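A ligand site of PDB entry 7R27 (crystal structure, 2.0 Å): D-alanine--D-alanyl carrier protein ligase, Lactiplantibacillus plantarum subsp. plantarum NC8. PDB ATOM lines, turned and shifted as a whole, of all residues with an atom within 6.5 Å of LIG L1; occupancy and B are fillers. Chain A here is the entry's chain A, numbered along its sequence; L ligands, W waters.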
ATOM      1  N   ASP A 198       6.436 -25.635 -33.959  1.00  0.00           N
ATOM      2  CA  ASP A 198       6.687 -26.561 -32.874  1.00  0.00           C
ATOM      3  C   ASP A 198       5.888 -26.209 -31.615  1.00  0.00           C
ATOM      4  O   ASP A 198       5.360 -27.102 -30.940  1.00  0.00           O
ATOM      5  CB  ASP A 198       8.181 -26.542 -32.578  1.00  0.00           C
ATOM      6  CG  ASP A 198       8.603 -27.672 -31.722  1.00  0.00           C
ATOM      7  OD1 ASP A 198       7.779 -28.587 -31.558  1.00  0.00           O
ATOM      8  OD2 ASP A 198       9.735 -27.626 -31.208  1.00  0.00           O
ATOM      9  N   PRO A 244       6.397 -15.187 -25.708  1.00  0.00           N
ATOM     10  CA  PRO A 244       6.321 -13.964 -24.877  1.00  0.00           C
ATOM     11  C   PRO A 244       5.800 -12.746 -25.628  1.00  0.00           C
ATOM     12  O   PRO A 244       5.069 -11.935 -25.046  1.00  0.00           O
ATOM     13  CB  PRO A 244       7.774 -13.772 -24.423  1.00  0.00           C
ATOM     14  CG  PRO A 244       8.386 -15.127 -24.466  1.00  0.00           C
ATOM     15  CD  PRO A 244       7.665 -15.922 -25.530  1.00  0.00           C
ATOM     16  N   PHE A 269       5.322 -20.146 -21.604  1.00  0.00           N
ATOM     17  CA  PHE A 269       5.993 -19.337 -22.600  1.00  0.00           C
ATOM     18  C   PHE A 269       7.223 -20.070 -23.133  1.00  0.00           C
ATOM     19  O   PHE A 269       7.920 -20.761 -22.373  1.00  0.00           O
ATOM     20  CB  PHE A 269       6.344 -17.959 -22.012  1.00  0.00           C
ATOM     21  CG  PHE A 269       5.114 -17.156 -21.639  1.00  0.00           C
ATOM     22  CD1 PHE A 269       4.195 -16.789 -22.624  1.00  0.00           C
ATOM     23  CD2 PHE A 269       4.851 -16.813 -20.326  1.00  0.00           C
ATOM     24  CE1 PHE A 269       3.054 -16.075 -22.311  1.00  0.00           C
ATOM     25  CE2 PHE A 269       3.714 -16.096 -19.998  1.00  0.00           C
ATOM     26  CZ  PHE A 269       2.816 -15.715 -21.002  1.00  0.00           C
ATOM     27  N   CYS A 270       7.451 -19.955 -24.442  1.00  0.00           N
ATOM     28  CA  CYS A 270       8.584 -20.557 -25.133  1.00  0.00           C
ATOM     29  C   CYS A 270       8.872 -19.770 -26.403  1.00  0.00           C
ATOM     30  O   CYS A 270       8.038 -18.998 -26.879  1.00  0.00           O
ATOM     31  CB  CYS A 270       8.325 -22.021 -25.475  1.00  0.00           C
ATOM     32  SG  CYS A 270       9.801 -23.041 -25.782  1.00  0.00           S
ATOM     33  N   GLY A 271      10.066 -19.982 -26.946  1.00  0.00           N
ATOM     34  CA  GLY A 271      10.406 -19.511 -28.266  1.00  0.00           C
ATOM     35  C   GLY A 271      11.124 -18.174 -28.294  1.00  0.00           C
ATOM     36  O   GLY A 271      11.817 -17.890 -29.277  1.00  0.00           O
ATOM     37  N   GLU A 272      10.960 -17.351 -27.265  1.00  0.00           N
ATOM     38  CA  GLU A 272      11.694 -16.096 -27.170  1.00  0.00           C
ATOM     39  C   GLU A 272      12.037 -15.827 -25.720  1.00  0.00           C
ATOM     40  O   GLU A 272      11.540 -16.508 -24.803  1.00  0.00           O
ATOM     41  CB  GLU A 272      10.893 -14.906 -27.720  1.00  0.00           C
ATOM     42  CG  GLU A 272      10.339 -15.086 -29.106  1.00  0.00           C
ATOM     43  CD  GLU A 272       9.105 -14.256 -29.325  1.00  0.00           C
ATOM     44  OE1 GLU A 272       8.513 -13.819 -28.317  1.00  0.00           O
ATOM     45  OE2 GLU A 272       8.725 -14.049 -30.496  1.00  0.00           O
ATOM     46  N   GLU A 273      12.878 -14.830 -25.525  1.00  0.00           N
ATOM     47  CA  GLU A 273      13.173 -14.353 -24.189  1.00  0.00           C
ATOM     48  C   GLU A 273      11.908 -13.794 -23.550  1.00  0.00           C
ATOM     49  O   GLU A 273      11.181 -13.001 -24.162  1.00  0.00           O
ATOM     50  CB  GLU A 273      14.250 -13.281 -24.238  1.00  0.00           C
ATOM     51  CG  GLU A 273      14.269 -12.328 -23.043  1.00  0.00           C
ATOM     52  CD  GLU A 273      15.020 -11.028 -23.341  1.00  0.00           C
ATOM     53  OE1 GLU A 273      14.541 -10.203 -24.154  1.00  0.00           O
ATOM     54  OE2 GLU A 273      16.119 -10.849 -22.764  1.00  0.00           O
ATOM     55  N   LEU A 274      11.626 -14.226 -22.329  1.00  0.00           N
ATOM     56  CA  LEU A 274      10.566 -13.631 -21.531  1.00  0.00           C
ATOM     57  C   LEU A 274      11.182 -12.494 -20.731  1.00  0.00           C
ATOM     58  O   LEU A 274      12.018 -12.738 -19.840  1.00  0.00           O
ATOM     59  CB  LEU A 274       9.925 -14.683 -20.628  1.00  0.00           C
ATOM     60  CG  LEU A 274       8.798 -14.212 -19.697  1.00  0.00           C
ATOM     61  CD1 LEU A 274       7.719 -13.466 -20.458  1.00  0.00           C
ATOM     62  CD2 LEU A 274       8.218 -15.415 -18.967  1.00  0.00           C
ATOM     63  N   ASN A 293       8.651 -20.100 -17.752  1.00  0.00           N
ATOM     64  CA  ASN A 293       9.528 -19.869 -18.878  1.00  0.00           C
ATOM     65  C   ASN A 293      10.101 -21.225 -19.269  1.00  0.00           C
ATOM     66  O   ASN A 293      10.443 -22.027 -18.395  1.00  0.00           O
ATOM     67  CB  ASN A 293      10.647 -18.894 -18.498  1.00  0.00           C
ATOM     68  CG  ASN A 293      11.352 -18.319 -19.692  1.00  0.00           C
ATOM     69  OD1 ASN A 293      10.796 -18.253 -20.781  1.00  0.00           O
ATOM     70  ND2 ASN A 293      12.591 -17.867 -19.489  1.00  0.00           N
ATOM     71  N   THR A 294      10.164 -21.495 -20.572  1.00  0.00           N
ATOM     72  CA  THR A 294      10.732 -22.734 -21.085  1.00  0.00           C
ATOM     73  C   THR A 294      11.556 -22.420 -22.327  1.00  0.00           C
ATOM     74  O   THR A 294      11.404 -21.353 -22.938  1.00  0.00           O
ATOM     75  CB  THR A 294       9.650 -23.765 -21.455  1.00  0.00           C
ATOM     76  OG1 THR A 294       8.859 -23.236 -22.534  1.00  0.00           O
ATOM     77  CG2 THR A 294       8.752 -24.065 -20.267  1.00  0.00           C
ATOM     78  N   TYR A 295      12.430 -23.364 -22.705  1.00  0.00           N
ATOM     79  CA  TYR A 295      13.245 -23.214 -23.896  1.00  0.00           C
ATOM     80  C   TYR A 295      13.677 -24.588 -24.392  1.00  0.00           C
ATOM     81  O   TYR A 295      13.894 -25.499 -23.593  1.00  0.00           O
ATOM     82  CB  TYR A 295      14.507 -22.371 -23.651  1.00  0.00           C
ATOM     83  CG  TYR A 295      15.727 -22.846 -24.426  1.00  0.00           C
ATOM     84  CD1 TYR A 295      15.926 -22.474 -25.761  1.00  0.00           C
ATOM     85  CD2 TYR A 295      16.677 -23.693 -23.851  1.00  0.00           C
ATOM     86  CE1 TYR A 295      17.028 -22.925 -26.491  1.00  0.00           C
ATOM     87  CE2 TYR A 295      17.776 -24.149 -24.573  1.00  0.00           C
ATOM     88  CZ  TYR A 295      17.956 -23.755 -25.890  1.00  0.00           C
ATOM     89  OH  TYR A 295      19.049 -24.175 -26.619  1.00  0.00           O
ATOM     90  N   GLY A 296      13.837 -24.704 -25.695  1.00  0.00           N
ATOM     91  CA  GLY A 296      14.379 -25.893 -26.291  1.00  0.00           C
ATOM     92  C   GLY A 296      14.263 -25.813 -27.789  1.00  0.00           C
ATOM     93  O   GLY A 296      13.274 -25.316 -28.339  1.00  0.00           O
ATOM     94  N   PRO A 297      15.279 -26.290 -28.500  1.00  0.00           N
ATOM     95  CA  PRO A 297      15.222 -26.240 -29.961  1.00  0.00           C
ATOM     96  C   PRO A 297      14.163 -27.207 -30.472  1.00  0.00           C
ATOM     97  O   PRO A 297      13.746 -28.144 -29.782  1.00  0.00           O
ATOM     98  CB  PRO A 297      16.638 -26.642 -30.409  1.00  0.00           C
ATOM     99  CG  PRO A 297      17.234 -27.366 -29.239  1.00  0.00           C
ATOM    100  CD  PRO A 297      16.533 -26.847 -27.983  1.00  0.00           C
ATOM    101  N   THR A 298      13.696 -26.915 -31.685  1.00  0.00           N
ATOM    102  CA  THR A 298      12.766 -27.824 -32.351  1.00  0.00           C
ATOM    103  C   THR A 298      13.374 -29.225 -32.486  1.00  0.00           C
ATOM    104  O   THR A 298      12.655 -30.220 -32.394  1.00  0.00           O
ATOM    105  CB  THR A 298      12.407 -27.242 -33.717  1.00  0.00           C
ATOM    106  OG1 THR A 298      11.854 -25.930 -33.545  1.00  0.00           O
ATOM    107  CG2 THR A 298      11.405 -28.124 -34.440  1.00  0.00           C
ATOM    108  N   GLU A 299      14.701 -29.297 -32.629  1.00  0.00           N
ATOM    109  CA  GLU A 299      15.361 -30.569 -32.864  1.00  0.00           C
ATOM    110  C   GLU A 299      15.357 -31.501 -31.656  1.00  0.00           C
ATOM    111  O   GLU A 299      15.665 -32.686 -31.809  1.00  0.00           O
ATOM    112  CB  GLU A 299      16.791 -30.317 -33.319  1.00  0.00           C
ATOM    113  CG  GLU A 299      16.902 -29.772 -34.756  1.00  0.00           C
ATOM    114  CD  GLU A 299      16.814 -28.261 -34.832  1.00  0.00           C
ATOM    115  OE1 GLU A 299      16.350 -27.643 -33.844  1.00  0.00           O
ATOM    116  OE2 GLU A 299      17.217 -27.684 -35.869  1.00  0.00           O
ATOM    117  N   VAL A 302      10.242 -29.467 -28.854  1.00  0.00           N
ATOM    118  CA  VAL A 302       9.471 -28.403 -28.204  1.00  0.00           C
ATOM    119  C   VAL A 302      10.253 -27.646 -27.134  1.00  0.00           C
ATOM    120  O   VAL A 302      10.587 -26.466 -27.302  1.00  0.00           O
ATOM    121  CB  VAL A 302       8.149 -28.924 -27.606  1.00  0.00           C
ATOM    122  CG1 VAL A 302       7.297 -27.741 -27.176  1.00  0.00           C
ATOM    123  CG2 VAL A 302       7.386 -29.769 -28.631  1.00  0.00           C
ATOM    124  N   LEU A 320      15.419 -13.159 -16.899  1.00  0.00           N
ATOM    125  CA  LEU A 320      14.872 -14.423 -16.417  1.00  0.00           C
ATOM    126  C   LEU A 320      15.708 -15.579 -16.952  1.00  0.00           C
ATOM    127  O   LEU A 320      16.010 -15.610 -18.148  1.00  0.00           O
ATOM    128  CB  LEU A 320      13.417 -14.576 -16.837  1.00  0.00           C
ATOM    129  CG  LEU A 320      12.506 -13.545 -16.173  1.00  0.00           C
ATOM    130  CD1 LEU A 320      11.091 -13.527 -16.737  1.00  0.00           C
ATOM    131  CD2 LEU A 320      12.496 -13.791 -14.685  1.00  0.00           C
ATOM    132  N   PRO A 321      16.132 -16.512 -16.104  1.00  0.00           N
ATOM    133  CA  PRO A 321      16.815 -17.704 -16.621  1.00  0.00           C
ATOM    134  C   PRO A 321      15.831 -18.554 -17.404  1.00  0.00           C
ATOM    135  O   PRO A 321      14.608 -18.424 -17.290  1.00  0.00           O
ATOM    136  CB  PRO A 321      17.290 -18.420 -15.354  1.00  0.00           C
ATOM    137  CG  PRO A 321      16.515 -17.852 -14.244  1.00  0.00           C
ATOM    138  CD  PRO A 321      16.016 -16.503 -14.641  1.00  0.00           C
ATOM    139  N   ILE A 322      16.399 -19.446 -18.240  1.00  0.00           N
ATOM    140  CA  ILE A 322      15.576 -20.391 -19.000  1.00  0.00           C
ATOM    141  C   ILE A 322      15.264 -21.653 -18.214  1.00  0.00           C
ATOM    142  O   ILE A 322      14.432 -22.469 -18.650  1.00  0.00           O
ATOM    143  CB  ILE A 322      16.209 -20.769 -20.356  1.00  0.00           C
ATOM    144  CG1 ILE A 322      17.602 -21.360 -20.171  1.00  0.00           C
ATOM    145  CG2 ILE A 322      16.293 -19.549 -21.253  1.00  0.00           C
ATOM    146  CD1 ILE A 322      18.336 -21.623 -21.472  1.00  0.00           C
ATOM    147  N   GLY A 383      22.297 -24.031 -31.603  1.00  0.00           N
ATOM    148  CA  GLY A 383      23.193 -22.931 -31.950  1.00  0.00           C
ATOM    149  C   GLY A 383      23.284 -21.914 -30.833  1.00  0.00           C
ATOM    150  O   GLY A 383      23.618 -20.753 -31.076  1.00  0.00           O
ATOM    151  N   ASP A 384      22.987 -22.333 -29.600  1.00  0.00           N
ATOM    152  CA  ASP A 384      22.715 -21.389 -28.513  1.00  0.00           C
ATOM    153  C   ASP A 384      23.883 -21.337 -27.549  1.00  0.00           C
ATOM    154  O   ASP A 384      24.443 -22.378 -27.178  1.00  0.00           O
ATOM    155  CB  ASP A 384      21.427 -21.756 -27.781  1.00  0.00           C
ATOM    156  CG  ASP A 384      20.231 -21.733 -28.702  1.00  0.00           C
ATOM    157  OD1 ASP A 384      20.230 -20.859 -29.594  1.00  0.00           O
ATOM    158  OD2 ASP A 384      19.326 -22.576 -28.572  1.00  0.00           O
ATOM    159  N   TYR A 396      20.125 -18.175 -21.133  1.00  0.00           N
ATOM    160  CA  TYR A 396      20.335 -17.992 -22.562  1.00  0.00           C
ATOM    161  C   TYR A 396      21.094 -16.685 -22.828  1.00  0.00           C
ATOM    162  O   TYR A 396      20.730 -15.632 -22.301  1.00  0.00           O
ATOM    163  CB  TYR A 396      19.003 -17.990 -23.309  1.00  0.00           C
ATOM    164  CG  TYR A 396      19.152 -17.735 -24.788  1.00  0.00           C
ATOM    165  CD1 TYR A 396      18.967 -16.460 -25.329  1.00  0.00           C
ATOM    166  CD2 TYR A 396      19.595 -18.749 -25.631  1.00  0.00           C
ATOM    167  CE1 TYR A 396      19.132 -16.234 -26.678  1.00  0.00           C
ATOM    168  CE2 TYR A 396      19.767 -18.537 -26.972  1.00  0.00           C
ATOM    169  CZ  TYR A 396      19.547 -17.271 -27.485  1.00  0.00           C
ATOM    170  OH  TYR A 396      19.731 -17.054 -28.831  1.00  0.00           O
ATOM    171  N   GLY A 398      22.621 -15.798 -26.199  1.00  0.00           N
ATOM    172  CA  GLY A 398      22.804 -15.463 -27.601  1.00  0.00           C
ATOM    173  C   GLY A 398      23.001 -16.707 -28.435  1.00  0.00           C
ATOM    174  O   GLY A 398      22.800 -17.841 -27.998  1.00  0.00           O
ATOM    175  N   ARG A 399      23.428 -16.484 -29.684  1.00  0.00           N
ATOM    176  CA  ARG A 399      23.631 -17.567 -30.635  1.00  0.00           C
ATOM    177  C   ARG A 399      25.065 -17.568 -31.149  1.00  0.00           C
ATOM    178  O   ARG A 399      25.703 -16.525 -31.252  1.00  0.00           O
ATOM    179  CB  ARG A 399      22.656 -17.462 -31.815  1.00  0.00           C
ATOM    180  CG  ARG A 399      21.355 -18.227 -31.579  1.00  0.00           C
ATOM    181  CD  ARG A 399      20.523 -18.409 -32.861  1.00  0.00           C
ATOM    182  NE  ARG A 399      20.936 -19.535 -33.697  1.00  0.00           N
ATOM    183  CZ  ARG A 399      20.907 -20.822 -33.342  1.00  0.00           C
ATOM    184  NH1 ARG A 399      20.487 -21.208 -32.150  1.00  0.00           N
ATOM    185  NH2 ARG A 399      21.316 -21.735 -34.218  1.00  0.00           N
HETATM  186  O1  LIG L   1      13.947 -22.609 -28.216  1.00  0.00           O
HETATM  187  O2  LIG L   1      13.047 -21.362 -30.256  1.00  0.00           O
HETATM  188  O3  LIG L   1      13.598 -23.785 -30.499  1.00  0.00           O
HETATM  189  O4  LIG L   1      15.317 -22.123 -30.250  1.00  0.00           O
HETATM  190  C1  LIG L   1      15.453 -21.089 -31.207  1.00  0.00           C
HETATM  191  C2  LIG L   1      15.887 -19.802 -30.545  1.00  0.00           C
HETATM  192  O5  LIG L   1      14.846 -19.308 -29.608  1.00  0.00           O
HETATM  193  C3  LIG L   1      17.149 -19.941 -29.686  1.00  0.00           C
HETATM  194  O6  LIG L   1      17.855 -18.693 -29.697  1.00  0.00           O
HETATM  195  C4  LIG L   1      16.537 -20.177 -28.321  1.00  0.00           C
HETATM  196  O7  LIG L   1      17.404 -20.101 -27.198  1.00  0.00           O
HETATM  197  C5  LIG L   1      15.454 -19.114 -28.340  1.00  0.00           C
HETATM  198  N1  LIG L   1      14.513 -19.214 -27.204  1.00  0.00           N
HETATM  199  C6  LIG L   1      13.436 -20.030 -27.078  1.00  0.00           C
HETATM  200  N2  LIG L   1      12.854 -19.902 -25.860  1.00  0.00           N
HETATM  201  C7  LIG L   1      13.589 -19.024 -25.156  1.00  0.00           C
HETATM  202  C8  LIG L   1      13.488 -18.465 -23.787  1.00  0.00           C
HETATM  203  N3  LIG L   1      12.469 -18.869 -22.997  1.00  0.00           N
HETATM  204  N4  LIG L   1      14.423 -17.560 -23.399  1.00  0.00           N
HETATM  205  C9  LIG L   1      15.420 -17.180 -24.240  1.00  0.00           C
HETATM  206  N5  LIG L   1      15.563 -17.651 -25.498  1.00  0.00           N
HETATM  207  C10 LIG L   1      14.690 -18.565 -26.025  1.00  0.00           C
HETATM  208  N1  LG2 L   2      10.990 -25.407 -30.676  1.00  0.00           N
HETATM  209  C1  LG2 L   2      10.346 -24.202 -30.170  1.00  0.00           C
HETATM  210  C2  LG2 L   2      10.642 -23.018 -31.099  1.00  0.00           C
HETATM  211  C3  LG2 L   2      10.818 -23.912 -28.759  1.00  0.00           C
HETATM  212  O1  LG2 L   2      11.123 -22.771 -28.435  1.00  0.00           O
HETATM  213  O   HOH W   1       9.575 -17.927 -23.425  1.00  0.00           O
HETATM  214  O   HOH W   2      14.136 -16.032 -20.672  1.00  0.00           O
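Water W2 lies within hydrogen-bond range of the side-chain amide nitrogen of Asn 293 (2.7 Å), a nitrogen (N4) of LIG L1 (3.1 Å) and the backbone carbonyl oxygen of Leu 320 (3.2 Å).
The side-chain hydroxyl of Tyr 396 lies within hydrogen-bond range of the backbone carbonyl oxygen of Gly 398.
OG1 of Thr 294 lies close to SG of Cys 270, at 3.4 Å.
The backbone carbonyl oxygen of Phe 269 is in hydrogen-bond range of the side-chain hydroxyl of Thr 294, 2.7 Å away.
ND2 of Asn 293 lies within hydrogen-bond range of O of Pro 321.
The side-chain carboxylate (OD2) of Asp 384 sits at hydrogen-bond distance from the side-chain hydroxyl (OH) of Tyr 295.
OD1 of Asp 384 is in salt-bridge range of NH1 of Arg 399.
The side-chain hydroxyl of Tyr 396 lies within hydrogen-bond range of an oxygen (O6) of LIG L1, at 2.6 Å.
N of Gly 296 sits close to O1 of LIG L1.
The backbone carbonyl oxygen (O) of Gly 296 is in hydrogen-bond range of an oxygen (O3) of LIG L1 (2.7 Å).
O of Thr 294 sits at hydrogen-bond distance from N3 of LIG L1, 2.7 Å away.
The side-chain amide oxygen of Asn 293 lies within hydrogen-bond range of a nitrogen (N3) of LIG L1 (2.8 Å).
The backbone NH (N) of Glu 272 sits at hydrogen-bond distance from a nitrogen (N2) of LIG L1 (3.5 Å).
The backbone carbonyl oxygen of Glu 272 sits close to a nitrogen (N3) of LIG L1 (3.1 Å).
N of Gly 271 sits at hydrogen-bond distance from N2 of LIG L1 (3.0 Å).
The side-chain carboxylate (OD1) of Asp 384 is in hydrogen-bond range of an oxygen (O6) of LIG L1 (3.2 Å).
An oxygen (O3) of LIG L1 sits at hydrogen-bond distance from the backbone NH (N) of Thr 298.
The backbone carbonyl oxygen (O) of Gly 296 sits close to a nitrogen (N1) of LG2 L2 (3.3 Å).
N of Gly 271 sits at hydrogen-bond distance from O1 of LG2 L2 (3.3 Å).
N1 of LG2 L2 lies close to N of Thr 298, 3.3 Å away.
OG1 of Thr 298 lies within hydrogen-bond range of N1 of LG2 L2, 3.0 Å away.
O1 of LG2 L2 sits at hydrogen-bond distance from SG of Cys 270, at 3.0 Å.
The side-chain carboxylate of Asp 198 is in salt-bridge range of a nitrogen (N1) of LG2 L2 (2.6 Å).
O2 of LIG L1 lies within hydrogen-bond range of O1 of LG2 L2.
Glu 273 touches LIG L1 (CA to N4, 3.5 Å).
Tyr 295 touches LIG L1.
Pro 297 touches LIG L1 (CA to O3, 3.0 Å).
Ile 322 touches LIG L1 (CG2 to N4, 3.5 Å).
Hydrophobic or aromatic side chains that line LIG L1: Tyr 295, Ile 322 and Tyr 396.
The nearest printed residue that does not touch LIG L1 is Arg 399 (4.001 Å).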
